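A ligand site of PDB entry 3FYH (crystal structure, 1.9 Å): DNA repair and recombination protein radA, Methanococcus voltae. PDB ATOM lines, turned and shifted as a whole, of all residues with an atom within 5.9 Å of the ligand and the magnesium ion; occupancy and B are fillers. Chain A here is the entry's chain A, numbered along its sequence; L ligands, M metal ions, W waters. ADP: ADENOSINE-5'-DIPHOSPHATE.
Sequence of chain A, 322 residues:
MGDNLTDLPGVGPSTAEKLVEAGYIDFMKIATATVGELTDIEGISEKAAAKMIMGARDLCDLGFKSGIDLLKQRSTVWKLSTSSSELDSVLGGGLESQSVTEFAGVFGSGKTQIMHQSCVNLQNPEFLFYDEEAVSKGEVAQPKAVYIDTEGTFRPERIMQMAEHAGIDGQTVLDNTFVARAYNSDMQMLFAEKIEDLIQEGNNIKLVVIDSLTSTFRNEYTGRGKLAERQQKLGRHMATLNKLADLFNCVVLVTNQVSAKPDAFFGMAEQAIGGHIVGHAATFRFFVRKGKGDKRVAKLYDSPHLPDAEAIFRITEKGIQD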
ATOM      1  N   GLY A 105      -6.747  -8.684 -11.605  1.00  0.00           N
ATOM      2  CA  GLY A 105      -5.824  -9.792 -11.769  1.00  0.00           C
ATOM      3  C   GLY A 105      -4.532  -9.469 -11.116  1.00  0.00           C
ATOM      4  O   GLY A 105      -4.336  -8.335 -10.717  1.00  0.00           O
ATOM      5  N   VAL A 106      -3.641 -10.461 -11.012  1.00  0.00           N
ATOM      6  CA  VAL A 106      -2.344 -10.244 -10.412  1.00  0.00           C
ATOM      7  C   VAL A 106      -1.457  -9.398 -11.308  1.00  0.00           C
ATOM      8  O   VAL A 106      -1.809  -9.171 -12.469  1.00  0.00           O
ATOM      9  CB  VAL A 106      -1.667 -11.597 -10.153  1.00  0.00           C
ATOM     10  CG1 VAL A 106      -2.462 -12.351  -9.060  1.00  0.00           C
ATOM     11  CG2 VAL A 106      -1.638 -12.417 -11.454  1.00  0.00           C
ATOM     12  N   PHE A 107      -0.324  -8.928 -10.769  1.00  0.00           N
ATOM     13  CA  PHE A 107       0.605  -8.098 -11.542  1.00  0.00           C
ATOM     14  C   PHE A 107       1.082  -8.911 -12.755  1.00  0.00           C
ATOM     15  O   PHE A 107       1.271 -10.125 -12.649  1.00  0.00           O
ATOM     16  CB  PHE A 107       1.820  -7.697 -10.677  1.00  0.00           C
ATOM     17  CG  PHE A 107       2.465  -6.350 -11.050  1.00  0.00           C
ATOM     18  CD1 PHE A 107       1.972  -5.147 -10.535  1.00  0.00           C
ATOM     19  CD2 PHE A 107       3.560  -6.295 -11.939  1.00  0.00           C
ATOM     20  CE1 PHE A 107       2.567  -3.894 -10.906  1.00  0.00           C
ATOM     21  CE2 PHE A 107       4.173  -5.063 -12.327  1.00  0.00           C
ATOM     22  CZ  PHE A 107       3.673  -3.866 -11.809  1.00  0.00           C
ATOM     23  N   GLY A 108       1.230  -8.258 -13.906  1.00  0.00           N
ATOM     24  CA  GLY A 108       1.681  -8.923 -15.113  1.00  0.00           C
ATOM     25  C   GLY A 108       0.652  -9.759 -15.844  1.00  0.00           C
ATOM     26  O   GLY A 108       1.000 -10.411 -16.815  1.00  0.00           O
ATOM     27  N   SER A 109      -0.619  -9.739 -15.437  1.00  0.00           N
ATOM     28  CA  SER A 109      -1.590 -10.565 -16.116  1.00  0.00           C
ATOM     29  C   SER A 109      -2.039  -9.949 -17.445  1.00  0.00           C
ATOM     30  O   SER A 109      -2.591 -10.652 -18.265  1.00  0.00           O
ATOM     31  CB  SER A 109      -2.808 -10.839 -15.213  1.00  0.00           C
ATOM     32  OG  SER A 109      -3.323  -9.622 -14.711  1.00  0.00           O
ATOM     33  N   GLY A 110      -1.799  -8.660 -17.652  1.00  0.00           N
ATOM     34  CA  GLY A 110      -2.198  -8.047 -18.914  1.00  0.00           C
ATOM     35  C   GLY A 110      -3.204  -6.880 -18.817  1.00  0.00           C
ATOM     36  O   GLY A 110      -3.730  -6.411 -19.839  1.00  0.00           O
ATOM     37  N   LYS A 111      -3.456  -6.398 -17.608  1.00  0.00           N
ATOM     38  CA  LYS A 111      -4.425  -5.320 -17.447  1.00  0.00           C
ATOM     39  C   LYS A 111      -4.030  -4.055 -18.234  1.00  0.00           C
ATOM     40  O   LYS A 111      -4.811  -3.522 -19.015  1.00  0.00           O
ATOM     41  CB  LYS A 111      -4.606  -5.006 -15.948  1.00  0.00           C
ATOM     42  CG  LYS A 111      -5.058  -6.232 -15.183  1.00  0.00           C
ATOM     43  CD  LYS A 111      -5.295  -5.942 -13.693  1.00  0.00           C
ATOM     44  CE  LYS A 111      -4.067  -5.416 -13.010  1.00  0.00           C
ATOM     45  NZ  LYS A 111      -3.019  -6.457 -12.935  1.00  0.00           N
ATOM     46  N   THR A 112      -2.805  -3.600 -18.034  1.00  0.00           N
ATOM     47  CA  THR A 112      -2.361  -2.402 -18.708  1.00  0.00           C
ATOM     48  C   THR A 112      -2.268  -2.635 -20.228  1.00  0.00           C
ATOM     49  O   THR A 112      -2.588  -1.728 -21.004  1.00  0.00           O
ATOM     50  CB  THR A 112      -1.030  -1.929 -18.077  1.00  0.00           C
ATOM     51  OG1 THR A 112      -1.299  -1.529 -16.729  1.00  0.00           O
ATOM     52  CG2 THR A 112      -0.426  -0.753 -18.848  1.00  0.00           C
ATOM     53  N   GLN A 113      -1.933  -3.859 -20.646  1.00  0.00           N
ATOM     54  CA  GLN A 113      -1.866  -4.177 -22.087  1.00  0.00           C
ATOM     55  C   GLN A 113      -3.249  -4.008 -22.730  1.00  0.00           C
ATOM     56  O   GLN A 113      -3.372  -3.444 -23.823  1.00  0.00           O
ATOM     57  CB  GLN A 113      -1.416  -5.626 -22.338  1.00  0.00           C
ATOM     58  CG  GLN A 113      -0.008  -5.958 -21.819  1.00  0.00           C
ATOM     59  CD  GLN A 113       0.998  -4.936 -22.273  1.00  0.00           C
ATOM     60  OE1 GLN A 113       1.288  -4.815 -23.463  1.00  0.00           O
ATOM     61  NE2 GLN A 113       1.527  -4.160 -21.315  1.00  0.00           N
ATOM     62  N   ILE A 114      -4.288  -4.511 -22.065  1.00  0.00           N
ATOM     63  CA  ILE A 114      -5.656  -4.404 -22.582  1.00  0.00           C
ATOM     64  C   ILE A 114      -6.055  -2.951 -22.676  1.00  0.00           C
ATOM     65  O   ILE A 114      -6.725  -2.565 -23.627  1.00  0.00           O
ATOM     66  CB  ILE A 114      -6.633  -5.240 -21.682  1.00  0.00           C
ATOM     67  CG1 ILE A 114      -6.234  -6.719 -21.836  1.00  0.00           C
ATOM     68  CG2 ILE A 114      -8.135  -5.046 -22.127  1.00  0.00           C
ATOM     69  CD1 ILE A 114      -6.929  -7.697 -20.894  1.00  0.00           C
ATOM     70  N   GLU A 151      -0.750   4.804 -12.290  1.00  0.00           N
ATOM     71  CA  GLU A 151       0.468   4.071 -11.993  1.00  0.00           C
ATOM     72  C   GLU A 151       1.744   4.592 -12.658  1.00  0.00           C
ATOM     73  O   GLU A 151       2.835   4.216 -12.245  1.00  0.00           O
ATOM     74  CB  GLU A 151       0.296   2.633 -12.456  1.00  0.00           C
ATOM     75  CG  GLU A 151      -1.032   2.041 -12.135  1.00  0.00           C
ATOM     76  CD  GLU A 151      -1.119   1.685 -10.673  1.00  0.00           C
ATOM     77  OE1 GLU A 151      -0.325   0.822 -10.231  1.00  0.00           O
ATOM     78  OE2 GLU A 151      -1.962   2.254  -9.951  1.00  0.00           O
ATOM     79  N   THR A 153       2.259   4.003 -15.859  1.00  0.00           N
ATOM     80  CA  THR A 153       2.643   2.964 -16.832  1.00  0.00           C
ATOM     81  C   THR A 153       2.141   3.145 -18.275  1.00  0.00           C
ATOM     82  O   THR A 153       2.237   2.215 -19.103  1.00  0.00           O
ATOM     83  CB  THR A 153       2.321   1.507 -16.316  1.00  0.00           C
ATOM     84  OG1 THR A 153       0.982   1.477 -15.761  1.00  0.00           O
ATOM     85  CG2 THR A 153       3.338   1.096 -15.225  1.00  0.00           C
ATOM     86  N   ARG A 158       4.442   1.482 -26.742  1.00  0.00           N
ATOM     87  CA  ARG A 158       3.593   0.316 -26.854  1.00  0.00           C
ATOM     88  C   ARG A 158       2.401   0.652 -27.742  1.00  0.00           C
ATOM     89  O   ARG A 158       1.958  -0.181 -28.516  1.00  0.00           O
ATOM     90  CB  ARG A 158       3.118  -0.157 -25.457  1.00  0.00           C
ATOM     91  CG  ARG A 158       2.359  -1.466 -25.493  1.00  0.00           C
ATOM     92  CD  ARG A 158       3.258  -2.616 -26.001  1.00  0.00           C
ATOM     93  NE  ARG A 158       2.725  -3.922 -25.632  1.00  0.00           N
ATOM     94  CZ  ARG A 158       2.729  -4.990 -26.417  1.00  0.00           C
ATOM     95  NH1 ARG A 158       2.238  -6.130 -25.984  1.00  0.00           N
ATOM     96  NH2 ARG A 158       3.208  -4.896 -27.651  1.00  0.00           N
ATOM     97  N   GLN A 161       3.703   0.446 -31.340  1.00  0.00           N
ATOM     98  CA  GLN A 161       3.914  -0.932 -31.756  1.00  0.00           C
ATOM     99  C   GLN A 161       2.602  -1.682 -32.029  1.00  0.00           C
ATOM    100  O   GLN A 161       2.466  -2.342 -33.064  1.00  0.00           O
ATOM    101  CB  GLN A 161       4.737  -1.671 -30.704  1.00  0.00           C
ATOM    102  CG  GLN A 161       4.949  -3.117 -30.978  1.00  0.00           C
ATOM    103  CD  GLN A 161       5.764  -3.799 -29.903  1.00  0.00           C
ATOM    104  OE1 GLN A 161       5.515  -3.620 -28.696  1.00  0.00           O
ATOM    105  NE2 GLN A 161       6.735  -4.612 -30.333  1.00  0.00           N
ATOM    106  N   ASP A 211      -6.583   3.263 -15.205  1.00  0.00           N
ATOM    107  CA  ASP A 211      -5.622   2.222 -14.857  1.00  0.00           C
ATOM    108  C   ASP A 211      -4.698   2.840 -13.785  1.00  0.00           C
ATOM    109  O   ASP A 211      -3.810   3.618 -14.139  1.00  0.00           O
ATOM    110  CB  ASP A 211      -4.835   1.876 -16.125  1.00  0.00           C
ATOM    111  CG  ASP A 211      -3.810   0.779 -15.888  1.00  0.00           C
ATOM    112  OD1 ASP A 211      -2.820   0.711 -16.654  1.00  0.00           O
ATOM    113  OD2 ASP A 211      -3.994  -0.036 -14.953  1.00  0.00           O
ATOM    114  N   GLN A 257      -5.965  -4.011  -9.320  1.00  0.00           N
ATOM    115  CA  GLN A 257      -4.809  -4.803  -8.995  1.00  0.00           C
ATOM    116  C   GLN A 257      -5.164  -5.563  -7.723  1.00  0.00           C
ATOM    117  O   GLN A 257      -5.241  -4.954  -6.655  1.00  0.00           O
ATOM    118  CB  GLN A 257      -3.619  -3.854  -8.798  1.00  0.00           C
ATOM    119  CG  GLN A 257      -2.301  -4.510  -8.360  1.00  0.00           C
ATOM    120  CD  GLN A 257      -1.720  -5.540  -9.337  1.00  0.00           C
ATOM    121  OE1 GLN A 257      -1.690  -6.724  -9.038  1.00  0.00           O
ATOM    122  NE2 GLN A 257      -1.264  -5.079 -10.521  1.00  0.00           N
ATOM    123  N   LYS A 290      -2.337 -15.621 -15.444  1.00  0.00           N
ATOM    124  CA  LYS A 290      -1.321 -16.044 -16.403  1.00  0.00           C
ATOM    125  C   LYS A 290      -1.453 -17.514 -16.752  1.00  0.00           C
ATOM    126  O   LYS A 290      -1.750 -18.342 -15.890  1.00  0.00           O
ATOM    127  CB  LYS A 290       0.074 -15.817 -15.843  1.00  0.00           C
ATOM    128  CG  LYS A 290       0.293 -14.439 -15.288  1.00  0.00           C
ATOM    129  CD  LYS A 290       1.761 -14.199 -15.039  1.00  0.00           C
ATOM    130  CE  LYS A 290       1.988 -12.847 -14.390  1.00  0.00           C
ATOM    131  NZ  LYS A 290       3.399 -12.427 -14.620  1.00  0.00           N
ATOM    132  N   ASP A 294       3.292 -16.938 -22.702  1.00  0.00           N
ATOM    133  CA  ASP A 294       2.522 -15.995 -23.491  1.00  0.00           C
ATOM    134  C   ASP A 294       1.006 -15.916 -23.192  1.00  0.00           C
ATOM    135  O   ASP A 294       0.360 -14.873 -23.441  1.00  0.00           O
ATOM    136  CB  ASP A 294       2.623 -16.432 -24.954  1.00  0.00           C
ATOM    137  CG  ASP A 294       3.008 -15.331 -25.839  1.00  0.00           C
ATOM    138  OD1 ASP A 294       2.895 -14.168 -25.369  1.00  0.00           O
ATOM    139  OD2 ASP A 294       3.421 -15.601 -26.990  1.00  0.00           O
ATOM    140  N   ARG A 296      -2.780 -16.157 -21.443  1.00  0.00           N
ATOM    141  CA  ARG A 296      -3.504 -15.499 -20.362  1.00  0.00           C
ATOM    142  C   ARG A 296      -4.931 -16.031 -20.391  1.00  0.00           C
ATOM    143  O   ARG A 296      -5.442 -16.397 -21.456  1.00  0.00           O
ATOM    144  CB  ARG A 296      -3.518 -13.974 -20.593  1.00  0.00           C
ATOM    145  CG  ARG A 296      -2.114 -13.302 -20.570  1.00  0.00           C
ATOM    146  CD  ARG A 296      -1.533 -13.338 -19.185  1.00  0.00           C
ATOM    147  NE  ARG A 296      -0.251 -12.635 -19.103  1.00  0.00           N
ATOM    148  CZ  ARG A 296       0.922 -13.134 -19.476  1.00  0.00           C
ATOM    149  NH1 ARG A 296       1.001 -14.377 -19.983  1.00  0.00           N
ATOM    150  NH2 ARG A 296       2.009 -12.403 -19.326  1.00  0.00           N
ATOM    151  N   ILE A 315      -0.495 -12.411 -25.069  1.00  0.00           N
ATOM    152  CA  ILE A 315       0.021 -11.066 -25.195  1.00  0.00           C
ATOM    153  C   ILE A 315       1.379 -11.194 -25.904  1.00  0.00           C
ATOM    154  O   ILE A 315       2.284 -11.874 -25.416  1.00  0.00           O
ATOM    155  CB  ILE A 315       0.208 -10.413 -23.847  1.00  0.00           C
ATOM    156  CG1 ILE A 315      -1.156 -10.265 -23.169  1.00  0.00           C
ATOM    157  CG2 ILE A 315       0.852  -9.014 -24.048  1.00  0.00           C
ATOM    158  CD1 ILE A 315      -1.071  -9.699 -21.744  1.00  0.00           C
ATOM    159  N   THR A 316       1.501 -10.549 -27.066  1.00  0.00           N
ATOM    160  CA  THR A 316       2.741 -10.662 -27.857  1.00  0.00           C
ATOM    161  C   THR A 316       3.206  -9.289 -28.276  1.00  0.00           C
ATOM    162  O   THR A 316       2.656  -8.286 -27.807  1.00  0.00           O
ATOM    163  CB  THR A 316       2.470 -11.481 -29.144  1.00  0.00           C
ATOM    164  OG1 THR A 316       1.695 -10.666 -30.034  1.00  0.00           O
ATOM    165  CG2 THR A 316       1.702 -12.791 -28.808  1.00  0.00           C
ATOM    166  N   GLU A 317       4.202  -9.187 -29.159  1.00  0.00           N
ATOM    167  CA  GLU A 317       4.599  -7.839 -29.615  1.00  0.00           C
ATOM    168  C   GLU A 317       3.481  -7.173 -30.404  1.00  0.00           C
ATOM    169  O   GLU A 317       3.451  -5.952 -30.531  1.00  0.00           O
ATOM    170  CB  GLU A 317       5.863  -7.882 -30.493  1.00  0.00           C
ATOM    171  CG  GLU A 317       6.363  -9.266 -30.821  1.00  0.00           C
ATOM    172  CD  GLU A 317       5.421 -10.067 -31.728  1.00  0.00           C
ATOM    173  OE1 GLU A 317       4.992  -9.537 -32.771  1.00  0.00           O
ATOM    174  OE2 GLU A 317       5.114 -11.236 -31.391  1.00  0.00           O
ATOM    175  N   LYS A 318       2.552  -7.953 -30.940  1.00  0.00           N
ATOM    176  CA  LYS A 318       1.464  -7.341 -31.696  1.00  0.00           C
ATOM    177  C   LYS A 318       0.396  -6.765 -30.776  1.00  0.00           C
ATOM    178  O   LYS A 318      -0.467  -5.990 -31.208  1.00  0.00           O
ATOM    179  CB  LYS A 318       0.806  -8.370 -32.603  1.00  0.00           C
ATOM    180  CG  LYS A 318       1.717  -8.892 -33.700  1.00  0.00           C
ATOM    181  CD  LYS A 318       1.115 -10.125 -34.298  1.00  0.00           C
ATOM    182  CE  LYS A 318       1.858 -10.544 -35.535  1.00  0.00           C
ATOM    183  NZ  LYS A 318       3.297 -10.651 -35.219  1.00  0.00           N
HETATM  184  PB  ADP L   1      -0.502  -5.741 -15.449  1.00  0.00           P
HETATM  185  O1B ADP L   1      -0.866  -4.376 -15.802  1.00  0.00           O
HETATM  186  O2B ADP L   1      -1.679  -6.606 -15.288  1.00  0.00           O
HETATM  187  O3B ADP L   1       0.377  -5.752 -14.154  1.00  0.00           O
HETATM  188  PA  ADP L   1       0.842  -5.686 -17.940  1.00  0.00           P
HETATM  189  O1A ADP L   1      -0.327  -5.157 -18.737  1.00  0.00           O
HETATM  190  O2A ADP L   1       1.761  -4.621 -17.648  1.00  0.00           O
HETATM  191  O3A ADP L   1       0.368  -6.401 -16.601  1.00  0.00           O
HETATM  192  O5' ADP L   1       1.516  -6.923 -18.786  1.00  0.00           O
HETATM  193  C5' ADP L   1       2.993  -7.210 -18.749  1.00  0.00           C
HETATM  194  C4' ADP L   1       3.265  -8.217 -19.602  1.00  0.00           C
HETATM  195  O4' ADP L   1       2.904  -7.760 -20.972  1.00  0.00           O
HETATM  196  C3' ADP L   1       4.812  -8.348 -19.718  1.00  0.00           C
HETATM  197  O3' ADP L   1       5.486  -8.802 -18.648  1.00  0.00           O
HETATM  198  C2' ADP L   1       5.076  -8.798 -21.138  1.00  0.00           C
HETATM  199  O2' ADP L   1       5.000 -10.316 -21.130  1.00  0.00           O
HETATM  200  C1' ADP L   1       3.871  -8.333 -21.896  1.00  0.00           C
HETATM  201  N9  ADP L   1       4.389  -7.396 -22.732  1.00  0.00           N
HETATM  202  C8  ADP L   1       4.547  -5.991 -22.531  1.00  0.00           C
HETATM  203  N7  ADP L   1       5.116  -5.466 -23.579  1.00  0.00           N
HETATM  204  C5  ADP L   1       5.359  -6.468 -24.485  1.00  0.00           C
HETATM  205  C6  ADP L   1       5.933  -6.505 -25.743  1.00  0.00           C
HETATM  206  N6  ADP L   1       6.414  -5.375 -26.333  1.00  0.00           N
HETATM  207  N1  ADP L   1       6.017  -7.744 -26.403  1.00  0.00           N
HETATM  208  C2  ADP L   1       5.529  -8.939 -25.819  1.00  0.00           C
HETATM  209  N3  ADP L   1       4.960  -8.951 -24.572  1.00  0.00           N
HETATM  210  C4  ADP L   1       4.902  -7.669 -23.956  1.00  0.00           C
HETATM  211 MG    MG M   1      -0.456  -2.454 -15.009  1.00  0.00          MG
HETATM  212  O   HOH W   1       3.994  -5.132 -16.506  1.00  0.00           O
HETATM  213  O   HOH W   2       4.346 -12.863 -20.517  1.00  0.00           O
HETATM  214  O   HOH W   3       4.141 -11.525 -23.428  1.00  0.00           O
HETATM  215  O   HOH W   4       0.045  -0.438 -14.300  1.00  0.00           O
HETATM  216  O   HOH W   5       0.348  -3.389 -13.327  1.00  0.00           O
HETATM  217  O   HOH W   6       1.414  -2.593 -16.076  1.00  0.00           O
HETATM  218  O   HOH W   7       8.667  -5.911 -28.524  1.00  0.00           O
HETATM  219  O   HOH W   8      -2.444  -2.140 -14.138  1.00  0.00           O
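N of Thr 112 sits at hydrogen-bond distance from O1A of the ligand, at 3.0 Å. The backbone NH (N) of Gly 108 is in hydrogen-bond range of an oxygen (O3B) of the ligand, at 2.7 Å. An oxygen (O2B) of the ligand lies within hydrogen-bond range of the backbone NH (N) of Lys 111, at 2.9 Å. The side-chain amino group of Lys 111 lies within salt-bridge range of an oxygen (O2B) of the ligand (2.7 Å). The backbone NH (N) of Gln 113 lies within hydrogen-bond range of an oxygen (O1A) of the ligand. The side-chain amide nitrogen (NE2) of Gln 113 lies close to an oxygen (O1A) of the ligand. The side-chain amide oxygen (OE1) of Gln 161 is in hydrogen-bond range of a nitrogen (N6) of the ligand, 3.1 Å away. An oxygen (O2B) of the ligand sits at hydrogen-bond distance from the backbone NH (N) of Gly 110. O2B of the ligand is in hydrogen-bond range of N of Ser 109, 3.3 Å away. The side-chain hydroxyl (OG) of Ser 109 is in hydrogen-bond range of an oxygen (O2B) of the ligand (3.5 Å).
OD1 of Asp 211 lies close to OG1 of Thr 112, at 2.7 Å. O of Val 106 is in hydrogen-bond range of NZ of Lys 111, 3.0 Å away. NZ of Lys 111 is in hydrogen-bond range of O of Gly 105, 3.2 Å away. The side-chain amide oxygen of Gln 161 is in hydrogen-bond range of the guanidinium group of Arg 158 (2.8 Å). OG of Ser 109 sits at hydrogen-bond distance from O of Val 106. The backbone carbonyl oxygen (O) of Thr 316 sits at hydrogen-bond distance from the guanidinium group (NH1) of Arg 158. The side-chain hydroxyl (OG1) of Thr 316 lies within hydrogen-bond range of the backbone NH (N) of Lys 318 (3.0 Å). OE1 of Glu 317 lies within salt-bridge range of NZ of Lys 318, 3.2 Å away.
NH2 of Arg 158 sits close to N6 of the ligand, at 3.5 Å. Merely in contact with the ligand: Thr 316, Glu 317, Phe 107, Ile 315 and Val 106. Hydrophobic or aromatic side chains that line the ligand: Phe 107 and Ile 315. Within 4 Å of the ligand: Val 106, Phe 107, Gly 108, Ser 109, Gly 110, Lys 111, Thr 112, Gln 113, Arg 158, Gln 161, Ile 315, Thr 316 and Glu 317.
Within 4 Å of the magnesium ion: Thr 112. The nearest printed residue that does not touch the magnesium ion is Thr 153 (4.3 Å).
The magnesium ion is bound by water W5, O1B of the ligand, OG1 of Thr 112, water W6, water W8 and water W4.
Water W2 lies within hydrogen-bond range of NH2 of Arg 296 and O2' of the ligand. Water W3 lies within hydrogen-bond range of O2' of the ligand (2.7 Å) and O of Ile 315 (2.7 Å). Water W7 bridges NE2 of Gln 161 and N6 of the ligand.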
